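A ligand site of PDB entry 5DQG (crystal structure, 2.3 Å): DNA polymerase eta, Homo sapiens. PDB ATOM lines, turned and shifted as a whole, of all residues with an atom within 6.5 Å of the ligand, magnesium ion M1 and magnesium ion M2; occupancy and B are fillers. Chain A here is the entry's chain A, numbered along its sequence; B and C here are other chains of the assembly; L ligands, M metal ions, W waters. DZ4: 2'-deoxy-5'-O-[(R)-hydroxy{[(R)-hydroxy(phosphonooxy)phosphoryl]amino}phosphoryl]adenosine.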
ATOM      1  N   ASP A  16     -19.072  -1.998   0.876  1.00  0.00           N
ATOM      2  CA  ASP A  16     -18.572  -1.483  -0.375  1.00  0.00           C
ATOM      3  C   ASP A  16     -17.062  -1.112  -0.294  1.00  0.00           C
ATOM      4  O   ASP A  16     -16.661  -0.322   0.540  1.00  0.00           O
ATOM      5  CB  ASP A  16     -19.376  -0.272  -0.751  1.00  0.00           C
ATOM      6  CG  ASP A  16     -18.995   0.291  -2.052  1.00  0.00           C
ATOM      7  OD1 ASP A  16     -19.688   0.007  -3.090  1.00  0.00           O
ATOM      8  OD2 ASP A  16     -18.014   1.012  -2.077  1.00  0.00           O
ATOM      9  N   MET A  17     -16.253  -1.690  -1.180  1.00  0.00           N
ATOM     10  CA  MET A  17     -14.825  -1.488  -1.207  1.00  0.00           C
ATOM     11  C   MET A  17     -14.486  -0.034  -1.513  1.00  0.00           C
ATOM     12  O   MET A  17     -15.119   0.609  -2.347  1.00  0.00           O
ATOM     13  CB  MET A  17     -14.174  -2.372  -2.279  1.00  0.00           C
ATOM     14  CG  MET A  17     -14.546  -3.834  -2.203  1.00  0.00           C
ATOM     15  SD  MET A  17     -14.329  -4.541  -0.568  1.00  0.00           S
ATOM     16  CE  MET A  17     -12.559  -4.499  -0.443  1.00  0.00           C
ATOM     17  N   ASP A  18     -13.509   0.492  -0.789  1.00  0.00           N
ATOM     18  CA  ASP A  18     -13.075   1.864  -0.988  1.00  0.00           C
ATOM     19  C   ASP A  18     -12.272   1.914  -2.274  1.00  0.00           C
ATOM     20  O   ASP A  18     -11.431   1.079  -2.494  1.00  0.00           O
ATOM     21  CB  ASP A  18     -12.249   2.336   0.208  1.00  0.00           C
ATOM     22  CG  ASP A  18     -13.059   2.410   1.469  1.00  0.00           C
ATOM     23  OD1 ASP A  18     -14.278   2.525   1.391  1.00  0.00           O
ATOM     24  OD2 ASP A  18     -12.461   2.347   2.551  1.00  0.00           O
ATOM     25  N   CYS A  19     -12.519   2.919  -3.073  1.00  0.00           N
ATOM     26  CA  CYS A  19     -11.899   3.115  -4.378  1.00  0.00           C
ATOM     27  C   CYS A  19     -11.335   1.822  -5.007  1.00  0.00           C
ATOM     28  O   CYS A  19     -10.147   1.687  -5.180  1.00  0.00           O
ATOM     29  CB  CYS A  19     -10.839   4.201  -4.287  1.00  0.00           C
ATOM     30  SG  CYS A  19      -9.546   3.945  -3.063  1.00  0.00           S
ATOM     31  N   PHE A  20     -12.217   0.884  -5.285  1.00  0.00           N
ATOM     32  CA  PHE A  20     -11.850  -0.526  -5.474  1.00  0.00           C
ATOM     33  C   PHE A  20     -10.783  -0.801  -6.551  1.00  0.00           C
ATOM     34  O   PHE A  20      -9.788  -1.443  -6.267  1.00  0.00           O
ATOM     35  CB  PHE A  20     -13.105  -1.354  -5.732  1.00  0.00           C
ATOM     36  CG  PHE A  20     -12.848  -2.826  -5.801  1.00  0.00           C
ATOM     37  CD1 PHE A  20     -11.975  -3.443  -4.894  1.00  0.00           C
ATOM     38  CD2 PHE A  20     -13.471  -3.619  -6.783  1.00  0.00           C
ATOM     39  CE1 PHE A  20     -11.721  -4.792  -4.968  1.00  0.00           C
ATOM     40  CE2 PHE A  20     -13.203  -4.992  -6.861  1.00  0.00           C
ATOM     41  CZ  PHE A  20     -12.335  -5.587  -5.952  1.00  0.00           C
ATOM     42  N   PHE A  21     -10.968  -0.327  -7.778  1.00  0.00           N
ATOM     43  CA  PHE A  21      -9.958  -0.607  -8.820  1.00  0.00           C
ATOM     44  C   PHE A  21      -8.601  -0.007  -8.452  1.00  0.00           C
ATOM     45  O   PHE A  21      -7.574  -0.650  -8.674  1.00  0.00           O
ATOM     46  CB  PHE A  21     -10.407  -0.167 -10.207  1.00  0.00           C
ATOM     47  CG  PHE A  21     -11.558  -0.987 -10.792  1.00  0.00           C
ATOM     48  CD1 PHE A  21     -12.380  -1.777 -10.004  1.00  0.00           C
ATOM     49  CD2 PHE A  21     -11.834  -0.916 -12.145  1.00  0.00           C
ATOM     50  CE1 PHE A  21     -13.450  -2.482 -10.555  1.00  0.00           C
ATOM     51  CE2 PHE A  21     -12.902  -1.602 -12.706  1.00  0.00           C
ATOM     52  CZ  PHE A  21     -13.714  -2.414 -11.901  1.00  0.00           C
ATOM     53  N   VAL A  22      -8.616   1.185  -7.867  1.00  0.00           N
ATOM     54  CA  VAL A  22      -7.422   1.829  -7.352  1.00  0.00           C
ATOM     55  C   VAL A  22      -6.679   0.948  -6.327  1.00  0.00           C
ATOM     56  O   VAL A  22      -5.478   0.760  -6.443  1.00  0.00           O
ATOM     57  CB  VAL A  22      -7.732   3.226  -6.744  1.00  0.00           C
ATOM     58  CG1 VAL A  22      -6.520   3.797  -6.059  1.00  0.00           C
ATOM     59  CG2 VAL A  22      -8.184   4.189  -7.832  1.00  0.00           C
ATOM     60  N   GLN A  41      -8.867   3.877 -18.548  1.00  0.00           N
ATOM     61  CA  GLN A  41      -9.011   2.976 -19.671  1.00  0.00           C
ATOM     62  C   GLN A  41      -8.934   3.756 -20.956  1.00  0.00           C
ATOM     63  O   GLN A  41      -9.597   4.806 -21.096  1.00  0.00           O
ATOM     64  CB  GLN A  41     -10.311   2.117 -19.597  1.00  0.00           C
ATOM     65  CG  GLN A  41     -11.614   2.882 -19.599  1.00  0.00           C
ATOM     66  CD  GLN A  41     -12.875   1.995 -19.433  1.00  0.00           C
ATOM     67  OE1 GLN A  41     -12.831   0.776 -19.261  1.00  0.00           O
ATOM     68  NE2 GLN A  41     -14.020   2.650 -19.460  1.00  0.00           N
ATOM     69  N   ILE A  51     -12.051   5.834 -14.370  1.00  0.00           N
ATOM     70  CA  ILE A  51     -13.127   5.058 -13.783  1.00  0.00           C
ATOM     71  C   ILE A  51     -12.998   4.780 -12.275  1.00  0.00           C
ATOM     72  O   ILE A  51     -13.940   4.271 -11.673  1.00  0.00           O
ATOM     73  CB  ILE A  51     -13.364   3.747 -14.523  1.00  0.00           C
ATOM     74  CG1 ILE A  51     -12.181   2.798 -14.403  1.00  0.00           C
ATOM     75  CG2 ILE A  51     -13.665   4.026 -15.996  1.00  0.00           C
ATOM     76  CD1 ILE A  51     -12.464   1.460 -15.050  1.00  0.00           C
ATOM     77  N   ALA A  52     -11.872   5.123 -11.659  1.00  0.00           N
ATOM     78  CA  ALA A  52     -11.732   5.017 -10.189  1.00  0.00           C
ATOM     79  C   ALA A  52     -10.615   5.925  -9.685  1.00  0.00           C
ATOM     80  O   ALA A  52      -9.638   6.136 -10.359  1.00  0.00           O
ATOM     81  CB  ALA A  52     -11.511   3.566  -9.741  1.00  0.00           C
ATOM     82  N   VAL A  53     -10.802   6.466  -8.478  1.00  0.00           N
ATOM     83  CA  VAL A  53     -10.003   7.594  -7.975  1.00  0.00           C
ATOM     84  C   VAL A  53      -9.651   7.426  -6.491  1.00  0.00           C
ATOM     85  O   VAL A  53     -10.543   7.271  -5.672  1.00  0.00           O
ATOM     86  CB  VAL A  53     -10.773   8.916  -8.128  1.00  0.00           C
ATOM     87  CG1 VAL A  53      -9.895  10.055  -7.697  1.00  0.00           C
ATOM     88  CG2 VAL A  53     -11.230   9.111  -9.553  1.00  0.00           C
ATOM     89  N   TYR A  55      -8.625   8.539  -2.675  1.00  0.00           N
ATOM     90  CA  TYR A  55      -9.130   9.668  -1.912  1.00  0.00           C
ATOM     91  C   TYR A  55      -8.136  10.820  -1.852  1.00  0.00           C
ATOM     92  O   TYR A  55      -8.544  11.947  -1.829  1.00  0.00           O
ATOM     93  CB  TYR A  55      -9.568   9.256  -0.487  1.00  0.00           C
ATOM     94  CG  TYR A  55     -10.894   8.524  -0.505  1.00  0.00           C
ATOM     95  CD1 TYR A  55     -10.966   7.194  -0.896  1.00  0.00           C
ATOM     96  CD2 TYR A  55     -12.079   9.195  -0.262  1.00  0.00           C
ATOM     97  CE1 TYR A  55     -12.173   6.524  -0.965  1.00  0.00           C
ATOM     98  CE2 TYR A  55     -13.305   8.540  -0.335  1.00  0.00           C
ATOM     99  CZ  TYR A  55     -13.339   7.182  -0.676  1.00  0.00           C
ATOM    100  OH  TYR A  55     -14.526   6.487  -0.729  1.00  0.00           O
ATOM    101  N   ARG A  58      -9.011  12.537  -5.057  1.00  0.00           N
ATOM    102  CA  ARG A  58     -10.310  13.193  -4.868  1.00  0.00           C
ATOM    103  C   ARG A  58     -10.197  14.584  -4.185  1.00  0.00           C
ATOM    104  O   ARG A  58     -10.919  15.509  -4.510  1.00  0.00           O
ATOM    105  CB  ARG A  58     -11.243  12.286  -4.065  1.00  0.00           C
ATOM    106  CG  ARG A  58     -11.623  10.981  -4.747  1.00  0.00           C
ATOM    107  CD  ARG A  58     -12.775  10.226  -4.067  1.00  0.00           C
ATOM    108  NE  ARG A  58     -12.762   8.804  -4.411  1.00  0.00           N
ATOM    109  CZ  ARG A  58     -13.701   7.896  -4.103  1.00  0.00           C
ATOM    110  NH1 ARG A  58     -14.809   8.200  -3.439  1.00  0.00           N
ATOM    111  NH2 ARG A  58     -13.527   6.629  -4.505  1.00  0.00           N
ATOM    112  N   ARG A  64     -14.517  10.356 -11.250  1.00  0.00           N
ATOM    113  CA  ARG A  64     -14.902   9.392 -12.259  1.00  0.00           C
ATOM    114  C   ARG A  64     -15.436  10.156 -13.467  1.00  0.00           C
ATOM    115  O   ARG A  64     -15.898  11.290 -13.295  1.00  0.00           O
ATOM    116  CB  ARG A  64     -16.012   8.482 -11.638  1.00  0.00           C
ATOM    117  CG  ARG A  64     -16.508   7.373 -12.530  1.00  0.00           C
ATOM    118  CD  ARG A  64     -17.504   6.416 -11.878  1.00  0.00           C
ATOM    119  NE  ARG A  64     -18.502   7.059 -11.002  1.00  0.00           N
ATOM    120  CZ  ARG A  64     -18.812   6.673  -9.755  1.00  0.00           C
ATOM    121  NH1 ARG A  64     -18.259   5.600  -9.174  1.00  0.00           N
ATOM    122  NH2 ARG A  64     -19.725   7.363  -9.076  1.00  0.00           N
ATOM    123  N   LEU A  92     -11.632  -6.541 -17.885  1.00  0.00           N
ATOM    124  CA  LEU A  92     -11.793  -6.330 -16.438  1.00  0.00           C
ATOM    125  C   LEU A  92     -11.547  -7.548 -15.564  1.00  0.00           C
ATOM    126  O   LEU A  92     -11.966  -7.561 -14.429  1.00  0.00           O
ATOM    127  CB  LEU A  92     -13.201  -5.810 -16.173  1.00  0.00           C
ATOM    128  CG  LEU A  92     -13.640  -4.575 -16.985  1.00  0.00           C
ATOM    129  CD1 LEU A  92     -15.034  -4.177 -16.521  1.00  0.00           C
ATOM    130  CD2 LEU A  92     -12.653  -3.449 -16.811  1.00  0.00           C
ATOM    131  N   SER A 116     -22.753  -5.514  -6.952  1.00  0.00           N
ATOM    132  CA  SER A 116     -21.926  -4.918  -7.976  1.00  0.00           C
ATOM    133  C   SER A 116     -20.580  -5.630  -7.942  1.00  0.00           C
ATOM    134  O   SER A 116     -20.404  -6.535  -7.142  1.00  0.00           O
ATOM    135  CB  SER A 116     -21.722  -3.407  -7.737  1.00  0.00           C
ATOM    136  OG  SER A 116     -20.709  -3.098  -6.762  1.00  0.00           O
ATOM    137  N   ILE A 117     -19.638  -5.231  -8.797  1.00  0.00           N
ATOM    138  CA  ILE A 117     -18.327  -5.852  -8.740  1.00  0.00           C
ATOM    139  C   ILE A 117     -17.634  -5.570  -7.391  1.00  0.00           C
ATOM    140  O   ILE A 117     -16.774  -6.352  -7.005  1.00  0.00           O
ATOM    141  CB  ILE A 117     -17.405  -5.384  -9.887  1.00  0.00           C
ATOM    142  CG1 ILE A 117     -16.304  -6.426 -10.142  1.00  0.00           C
ATOM    143  CG2 ILE A 117     -16.842  -3.989  -9.633  1.00  0.00           C
ATOM    144  CD1 ILE A 117     -15.430  -6.082 -11.353  1.00  0.00           C
ATOM    145  N   ASP A 118     -18.024  -4.490  -6.671  1.00  0.00           N
ATOM    146  CA  ASP A 118     -17.354  -4.174  -5.397  1.00  0.00           C
ATOM    147  C   ASP A 118     -18.237  -4.083  -4.147  1.00  0.00           C
ATOM    148  O   ASP A 118     -17.801  -3.552  -3.105  1.00  0.00           O
ATOM    149  CB  ASP A 118     -16.532  -2.873  -5.556  1.00  0.00           C
ATOM    150  CG  ASP A 118     -17.338  -1.622  -5.227  1.00  0.00           C
ATOM    151  OD1 ASP A 118     -18.517  -1.515  -5.626  1.00  0.00           O
ATOM    152  OD2 ASP A 118     -16.780  -0.740  -4.566  1.00  0.00           O
ATOM    153  N   GLU A 119     -19.449  -4.607  -4.209  1.00  0.00           N
ATOM    154  CA  GLU A 119     -20.316  -4.563  -3.048  1.00  0.00           C
ATOM    155  C   GLU A 119     -21.315  -5.689  -2.960  1.00  0.00           C
ATOM    156  O   GLU A 119     -21.744  -6.221  -3.974  1.00  0.00           O
ATOM    157  CB  GLU A 119     -21.024  -3.218  -2.958  1.00  0.00           C
ATOM    158  CG  GLU A 119     -22.121  -2.961  -3.933  1.00  0.00           C
ATOM    159  CD  GLU A 119     -22.281  -1.470  -4.230  1.00  0.00           C
ATOM    160  OE1 GLU A 119     -21.484  -0.931  -5.000  1.00  0.00           O
ATOM    161  OE2 GLU A 119     -23.227  -0.848  -3.690  1.00  0.00           O
ATOM    162  N   SER A 216     -15.797   0.155   3.361  1.00  0.00           N
ATOM    163  CA  SER A 216     -16.767   0.771   4.249  1.00  0.00           C
ATOM    164  C   SER A 216     -18.023  -0.089   4.290  1.00  0.00           C
ATOM    165  O   SER A 216     -18.202  -0.964   3.447  1.00  0.00           O
ATOM    166  CB  SER A 216     -17.081   2.171   3.782  1.00  0.00           C
ATOM    167  OG  SER A 216     -15.859   2.883   3.672  1.00  0.00           O
ATOM    168  N   LYS A 234     -17.485   6.908   4.576  1.00  0.00           N
ATOM    169  CA  LYS A 234     -16.411   6.473   3.709  1.00  0.00           C
ATOM    170  C   LYS A 234     -15.236   7.458   3.766  1.00  0.00           C
ATOM    171  O   LYS A 234     -15.465   8.656   3.797  1.00  0.00           O
ATOM    172  CB  LYS A 234     -16.888   6.393   2.228  1.00  0.00           C
ATOM    173  CG  LYS A 234     -17.275   5.013   1.783  1.00  0.00           C
ATOM    174  CD  LYS A 234     -17.544   4.944   0.269  1.00  0.00           C
ATOM    175  CE  LYS A 234     -17.907   3.487  -0.133  1.00  0.00           C
ATOM    176  NZ  LYS A 234     -16.749   2.538  -0.224  1.00  0.00           N
ATOM    177  N   PRO A 235     -13.994   6.973   3.680  1.00  0.00           N
ATOM    178  CA  PRO A 235     -13.454   5.616   3.530  1.00  0.00           C
ATOM    179  C   PRO A 235     -13.109   4.889   4.831  1.00  0.00           C
ATOM    180  O   PRO A 235     -12.971   5.511   5.831  1.00  0.00           O
ATOM    181  CB  PRO A 235     -12.130   5.874   2.757  1.00  0.00           C
ATOM    182  CG  PRO A 235     -11.654   7.184   3.320  1.00  0.00           C
ATOM    183  CD  PRO A 235     -12.933   7.978   3.458  1.00  0.00           C
ATOM    184  P    DT B   8     -24.946   3.308  -7.474  1.00  0.00           P
ATOM    185  OP1  DT B   8     -24.763   3.469  -6.006  1.00  0.00           O
ATOM    186  OP2  DT B   8     -24.792   4.481  -8.404  1.00  0.00           O
ATOM    187  O5'  DT B   8     -23.872   2.265  -8.022  1.00  0.00           O
ATOM    188  C5'  DT B   8     -23.863   0.906  -7.577  1.00  0.00           C
ATOM    189  C4'  DT B   8     -22.616   0.284  -8.145  1.00  0.00           C
ATOM    190  O4'  DT B   8     -22.737   0.243  -9.574  1.00  0.00           O
ATOM    191  C3'  DT B   8     -21.346   1.078  -7.841  1.00  0.00           C
ATOM    192  O3'  DT B   8     -20.328   0.253  -7.269  1.00  0.00           O
ATOM    193  C2'  DT B   8     -20.960   1.721  -9.161  1.00  0.00           C
ATOM    194  C1'  DT B   8     -21.591   0.816 -10.186  1.00  0.00           C
ATOM    195  N1   DT B   8     -22.022   1.503 -11.414  1.00  0.00           N
ATOM    196  C2   DT B   8     -21.587   1.026 -12.632  1.00  0.00           C
ATOM    197  O2   DT B   8     -20.870   0.049 -12.752  1.00  0.00           O
ATOM    198  N3   DT B   8     -22.074   1.721 -13.720  1.00  0.00           N
ATOM    199  C4   DT B   8     -22.932   2.801 -13.704  1.00  0.00           C
ATOM    200  O4   DT B   8     -23.269   3.327 -14.755  1.00  0.00           O
ATOM    201  C5   DT B   8     -23.337   3.252 -12.391  1.00  0.00           C
ATOM    202  C7   DT B   8     -24.252   4.421 -12.273  1.00  0.00           C
ATOM    203  C6   DT B   8     -22.883   2.576 -11.324  1.00  0.00           C
ATOM    204  P    DT C   3     -18.082  12.701 -23.813  1.00  0.00           P
ATOM    205  OP1  DT C   3     -18.930  13.839 -24.242  1.00  0.00           O
ATOM    206  OP2  DT C   3     -17.132  12.885 -22.680  1.00  0.00           O
ATOM    207  O5'  DT C   3     -19.094  11.501 -23.506  1.00  0.00           O
ATOM    208  C5'  DT C   3     -18.954  10.677 -22.321  1.00  0.00           C
ATOM    209  C4'  DT C   3     -17.816   9.700 -22.501  1.00  0.00           C
ATOM    210  O4'  DT C   3     -17.194   9.431 -21.225  1.00  0.00           O
ATOM    211  C3'  DT C   3     -18.194   8.345 -23.091  1.00  0.00           C
ATOM    212  O3'  DT C   3     -17.198   7.927 -24.021  1.00  0.00           O
ATOM    213  C2'  DT C   3     -18.268   7.439 -21.873  1.00  0.00           C
ATOM    214  C1'  DT C   3     -17.249   8.044 -20.909  1.00  0.00           C
ATOM    215  N1   DT C   3     -17.588   7.917 -19.459  1.00  0.00           N
ATOM    216  C2   DT C   3     -16.676   7.353 -18.571  1.00  0.00           C
ATOM    217  O2   DT C   3     -15.578   6.947 -18.905  1.00  0.00           O
ATOM    218  N3   DT C   3     -17.115   7.287 -17.267  1.00  0.00           N
ATOM    219  C4   DT C   3     -18.328   7.736 -16.766  1.00  0.00           C
ATOM    220  O4   DT C   3     -18.573   7.621 -15.568  1.00  0.00           O
ATOM    221  C5   DT C   3     -19.228   8.326 -17.750  1.00  0.00           C
ATOM    222  C7   DT C   3     -20.552   8.851 -17.299  1.00  0.00           C
ATOM    223  C6   DT C   3     -18.816   8.378 -19.026  1.00  0.00           C
ATOM    224  C1  5EJ C   4     -22.025   5.242 -16.969  1.00  0.00           C
ATOM    225  C2  5EJ C   4     -17.868   3.491 -18.623  1.00  0.00           C
ATOM    226  P   5EJ C   4     -17.564   6.738 -25.188  1.00  0.00           P
ATOM    227  OP1 5EJ C   4     -16.884   7.148 -26.428  1.00  0.00           O
ATOM    228  O5' 5EJ C   4     -16.919   5.418 -24.557  1.00  0.00           O
ATOM    229  C5' 5EJ C   4     -15.785   5.448 -23.665  1.00  0.00           C
ATOM    230  C4' 5EJ C   4     -15.733   4.226 -22.760  1.00  0.00           C
ATOM    231  C3' 5EJ C   4     -16.525   3.034 -23.257  1.00  0.00           C
ATOM    232  O3' 5EJ C   4     -15.699   1.891 -23.215  1.00  0.00           O
ATOM    233  C2' 5EJ C   4     -17.681   2.842 -22.318  1.00  0.00           C
ATOM    234  C1' 5EJ C   4     -17.082   3.382 -21.038  1.00  0.00           C
ATOM    235  O4' 5EJ C   4     -16.299   4.499 -21.484  1.00  0.00           O
ATOM    236  N1  5EJ C   4     -18.046   3.826 -20.013  1.00  0.00           N
ATOM    237  C6  5EJ C   4     -19.079   4.587 -20.386  1.00  0.00           C
ATOM    238  C5  5EJ C   4     -19.998   5.069 -19.465  1.00  0.00           C
ATOM    239  C7  5EJ C   4     -21.156   5.919 -19.988  1.00  0.00           C
ATOM    240  C4  5EJ C   4     -19.792   4.699 -18.022  1.00  0.00           C
ATOM    241  N3  5EJ C   4     -18.716   3.936 -17.681  1.00  0.00           N
ATOM    242  O2  5EJ C   4     -16.921   2.781 -18.257  1.00  0.00           O
ATOM    243  O4  5EJ C   4     -20.589   5.113 -16.979  1.00  0.00           O
ATOM    244  OP2 5EJ C   4     -19.036   6.674 -25.372  1.00  0.00           O
ATOM    245  C3  5EJ C   4     -22.500   6.348 -16.039  1.00  0.00           C
ATOM    246  P    DA C   5     -16.246   0.432 -23.786  1.00  0.00           P
ATOM    247  OP1  DA C   5     -15.030  -0.183 -24.356  1.00  0.00           O
ATOM    248  OP2  DA C   5     -17.481   0.583 -24.583  1.00  0.00           O
ATOM    249  O5'  DA C   5     -16.572  -0.369 -22.456  1.00  0.00           O
ATOM    250  C5'  DA C   5     -15.499  -0.767 -21.594  1.00  0.00           C
ATOM    251  C4'  DA C   5     -15.970  -1.694 -20.489  1.00  0.00           C
ATOM    252  O4'  DA C   5     -16.820  -0.962 -19.577  1.00  0.00           O
ATOM    253  C3'  DA C   5     -16.790  -2.899 -20.959  1.00  0.00           C
ATOM    254  O3'  DA C   5     -16.425  -4.014 -20.133  1.00  0.00           O
ATOM    255  C2'  DA C   5     -18.215  -2.439 -20.743  1.00  0.00           C
ATOM    256  C1'  DA C   5     -18.053  -1.641 -19.463  1.00  0.00           C
ATOM    257  N9   DA C   5     -19.098  -0.644 -19.235  1.00  0.00           N
ATOM    258  C8   DA C   5     -19.691   0.173 -20.157  1.00  0.00           C
ATOM    259  N7   DA C   5     -20.586   0.988 -19.643  1.00  0.00           N
ATOM    260  C5   DA C   5     -20.571   0.681 -18.292  1.00  0.00           C
ATOM    261  C6   DA C   5     -21.286   1.201 -17.206  1.00  0.00           C
ATOM    262  N6   DA C   5     -22.213   2.150 -17.321  1.00  0.00           N
ATOM    263  N1   DA C   5     -21.028   0.689 -15.988  1.00  0.00           N
ATOM    264  C2   DA C   5     -20.109  -0.280 -15.882  1.00  0.00           C
ATOM    265  N3   DA C   5     -19.379  -0.851 -16.830  1.00  0.00           N
ATOM    266  C4   DA C   5     -19.660  -0.322 -18.030  1.00  0.00           C
HETATM  267  N1  DZ4 L   1     -17.760   2.636 -15.454  1.00  0.00           N
HETATM  268  C2  DZ4 L   1     -16.847   1.660 -15.285  1.00  0.00           C
HETATM  269  N3  DZ4 L   1     -16.471   1.161 -14.078  1.00  0.00           N
HETATM  270  C4  DZ4 L   1     -17.050   1.668 -12.986  1.00  0.00           C
HETATM  271  C5  DZ4 L   1     -18.093   2.708 -13.067  1.00  0.00           C
HETATM  272  C6  DZ4 L   1     -18.435   3.185 -14.440  1.00  0.00           C
HETATM  273  N6  DZ4 L   1     -19.353   4.140 -14.650  1.00  0.00           N
HETATM  274  N7  DZ4 L   1     -18.485   2.980 -11.816  1.00  0.00           N
HETATM  275  C8  DZ4 L   1     -17.748   2.209 -10.993  1.00  0.00           C
HETATM  276  N9  DZ4 L   1     -16.913   1.403 -11.697  1.00  0.00           N
HETATM  277  PA  DZ4 L   1     -17.918   2.375  -6.720  1.00  0.00           P
HETATM  278  PB  DZ4 L   1     -15.256   3.080  -5.761  1.00  0.00           P
HETATM  279  PG  DZ4 L   1     -15.917   4.303  -3.308  1.00  0.00           P
HETATM  280  C1' DZ4 L   1     -15.977   0.391 -11.173  1.00  0.00           C
HETATM  281  O1A DZ4 L   1     -19.215   3.135  -7.241  1.00  0.00           O
HETATM  282  O1B DZ4 L   1     -14.122   3.204  -6.717  1.00  0.00           O
HETATM  283  O1G DZ4 L   1     -16.640   5.643  -3.504  1.00  0.00           O
HETATM  284  C2' DZ4 L   1     -14.675   1.007 -10.707  1.00  0.00           C
HETATM  285  O2A DZ4 L   1     -17.996   1.615  -5.454  1.00  0.00           O
HETATM  286  O2B DZ4 L   1     -15.405   1.567  -5.207  1.00  0.00           O
HETATM  287  O2G DZ4 L   1     -14.854   4.355  -2.230  1.00  0.00           O
HETATM  288  C3' DZ4 L   1     -14.876   1.208  -9.240  1.00  0.00           C
HETATM  289  O3' DZ4 L   1     -13.636   1.198  -8.511  1.00  0.00           O
HETATM  290  N3A DZ4 L   1     -16.702   3.559  -6.574  1.00  0.00           N
HETATM  291  O3B DZ4 L   1     -15.092   4.253  -4.696  1.00  0.00           O
HETATM  292  O3G DZ4 L   1     -16.786   3.092  -3.288  1.00  0.00           O
HETATM  293  C4' DZ4 L   1     -15.770   0.032  -8.912  1.00  0.00           C
HETATM  294  O4' DZ4 L   1     -16.609  -0.209 -10.055  1.00  0.00           O
HETATM  295  C5' DZ4 L   1     -16.621   0.228  -7.677  1.00  0.00           C
HETATM  296  O5' DZ4 L   1     -17.471   1.352  -7.868  1.00  0.00           O
HETATM  297 MG    MG M   1     -16.790   1.098  -3.649  1.00  0.00          MG
HETATM  298 MG    MG M   2     -19.688   0.282  -5.098  1.00  0.00          MG
HETATM  299  O   HOH W   1     -14.880   0.059 -17.527  1.00  0.00           O
HETATM  300  O   HOH W   2     -18.084   7.890  -1.687  1.00  0.00           O
HETATM  301  O   HOH W   3     -20.519   5.184 -12.246  1.00  0.00           O
HETATM  302  O   HOH W   4     -20.722   1.987  -4.847  1.00  0.00           O
HETATM  303  O   HOH W   5     -13.289   5.642  -7.315  1.00  0.00           O
HETATM  304  O   HOH W   6     -17.321   6.371  -5.844  1.00  0.00           O
HETATM  305  O   HOH W   7     -19.467   4.045  -3.593  1.00  0.00           O
HETATM  306  O   HOH W   8     -18.480  -1.689 -12.492  1.00  0.00           O
HETATM  307  O   HOH W   9     -16.004   4.760  -9.601  1.00  0.00           O
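An oxygen (O2G) of the ligand is in hydrogen-bond range of the side-chain hydroxyl of Tyr 55, 2.6 Å away.
O4 of 5EJ 4 of chain C lies within hydrogen-bond range of N6 of the ligand, 2.8 Å away.
An oxygen (O1G) of the ligand is in salt-bridge range of the guanidinium group (NH1) of Arg 58 (3.1 Å).
O2G of the ligand sits at hydrogen-bond distance from N of Cys 19, at 2.9 Å.
An oxygen (O2G) of the ligand lies within salt-bridge range of the side-chain amino group (NZ) of Lys 234.
O3' of the ligand sits at hydrogen-bond distance from N of Phe 21, at 3.2 Å.
The backbone NH (N) of Phe 20 is in hydrogen-bond range of an oxygen (O1B) of the ligand, 3.3 Å away.
An oxygen (O1A) of the ligand lies within salt-bridge range of the guanidinium group (NH1) of Arg 64, at 3.3 Å.
The side-chain amino group (NZ) of Lys 234 lies within hydrogen-bond range of the backbone carbonyl oxygen (O) of Asp 16, at 3.0 Å.
The backbone NH (N) of Asp 118 lies within hydrogen-bond range of the side-chain hydroxyl (OG) of Ser 116 (3.0 Å).
The side-chain hydroxyl (OG) of Ser 116 lies close to the backbone NH (N) of Glu 119, at 3.2 Å.
The side-chain amino group (NZ) of Lys 234 lies close to the backbone carbonyl oxygen (O) of Met 17, 3.3 Å away.
N3 of DT 8 of chain B lies close to N1 of DA 5 of chain C.
The backbone carbonyl oxygen of Val 53 is in hydrogen-bond range of the guanidinium group of Arg 58.
NZ of Lys 234 lies within salt-bridge range of OD1 of Asp 18, at 3.0 Å.
The side-chain carboxylate of Asp 18 is in hydrogen-bond range of the side-chain hydroxyl of Ser 216 (2.8 Å).
Asp 18 touches the ligand.
Ile 51 touches the ligand (O to C2', 3.5 Å).
Ala 52 touches the ligand.
Ile 117 touches the ligand.
DT 3 of chain C touches the ligand.
C2 of DA 5 of chain C touches N1 of the ligand, 3.8 Å away.
Of the 26 residues printed, 18 come within 4 Å of the ligand.
Merely in contact with magnesium ion M1: Lys 234 (3.7 Å).
Within 4 Å of magnesium ion M1: Asp 16, Met 17, Asp 118 and Lys 234.
Along chain A the residues within 4 Å of magnesium ion M1 span positions 16 to 234.
Residues that only touch magnesium ion M2: Ser 116.
Within 4 Å of magnesium ion M2: Asp 16, Ser 116, Asp 118, Glu 119 and DT 8 of chain B.
The nearest printed residue that does not touch magnesium ion M2 is Met 17 (5.3 Å).
Magnesium ion M1 is bound by the side-chain carboxylate of Asp 16 (2.0 Å), an oxygen (O3G) of the ligand (2.0 Å), the side-chain carboxylate of Asp 118 (2.1 Å), an oxygen (O2B) of the ligand (2.1 Å), the backbone carbonyl oxygen of Met 17 (2.2 Å) and an oxygen (O2A) of the ligand (2.2 Å).
Magnesium ion M1 has six donor atoms within binding distance.
Magnesium ion M2 is bound by water W4, at 2.0 Å.
The side-chain carboxylate (OD1) of Asp 16 binds magnesium ion M2 (2.0 Å).
The side-chain carboxylate (OE1) of Glu 119 binds magnesium ion M2 (2.2 Å).
Magnesium ion M2 is bound by an oxygen (O2A) of the ligand (2.2 Å).
OD1 of Asp 118 is bound to magnesium ion M2 (2.2 Å).
O3' of DT 8 of chain B binds magnesium ion M2, at 2.3 Å.
Magnesium ion M2 has six donor atoms within binding distance.
Water W5 lies within hydrogen-bond range of O1B of the ligand (2.6 Å), N of Val 53 (2.9 Å) and NH2 of Arg 58 (3.0 Å).
Water W3 bridges N6 of the ligand (2.9 Å) and NE of Arg 64 (3.0 Å).
Water W9 lies within hydrogen-bond range of the guanidinium group (NH1) of Arg 64 (2.4 Å), the backbone carbonyl oxygen (O) of Ile 51 (3.0 Å) and a nitrogen (N3A) of the ligand (3.3 Å).
Water W8 lies within hydrogen-bond range of O2 of DT 8 of chain B (3.0 Å) and O4' of the ligand (3.4 Å).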
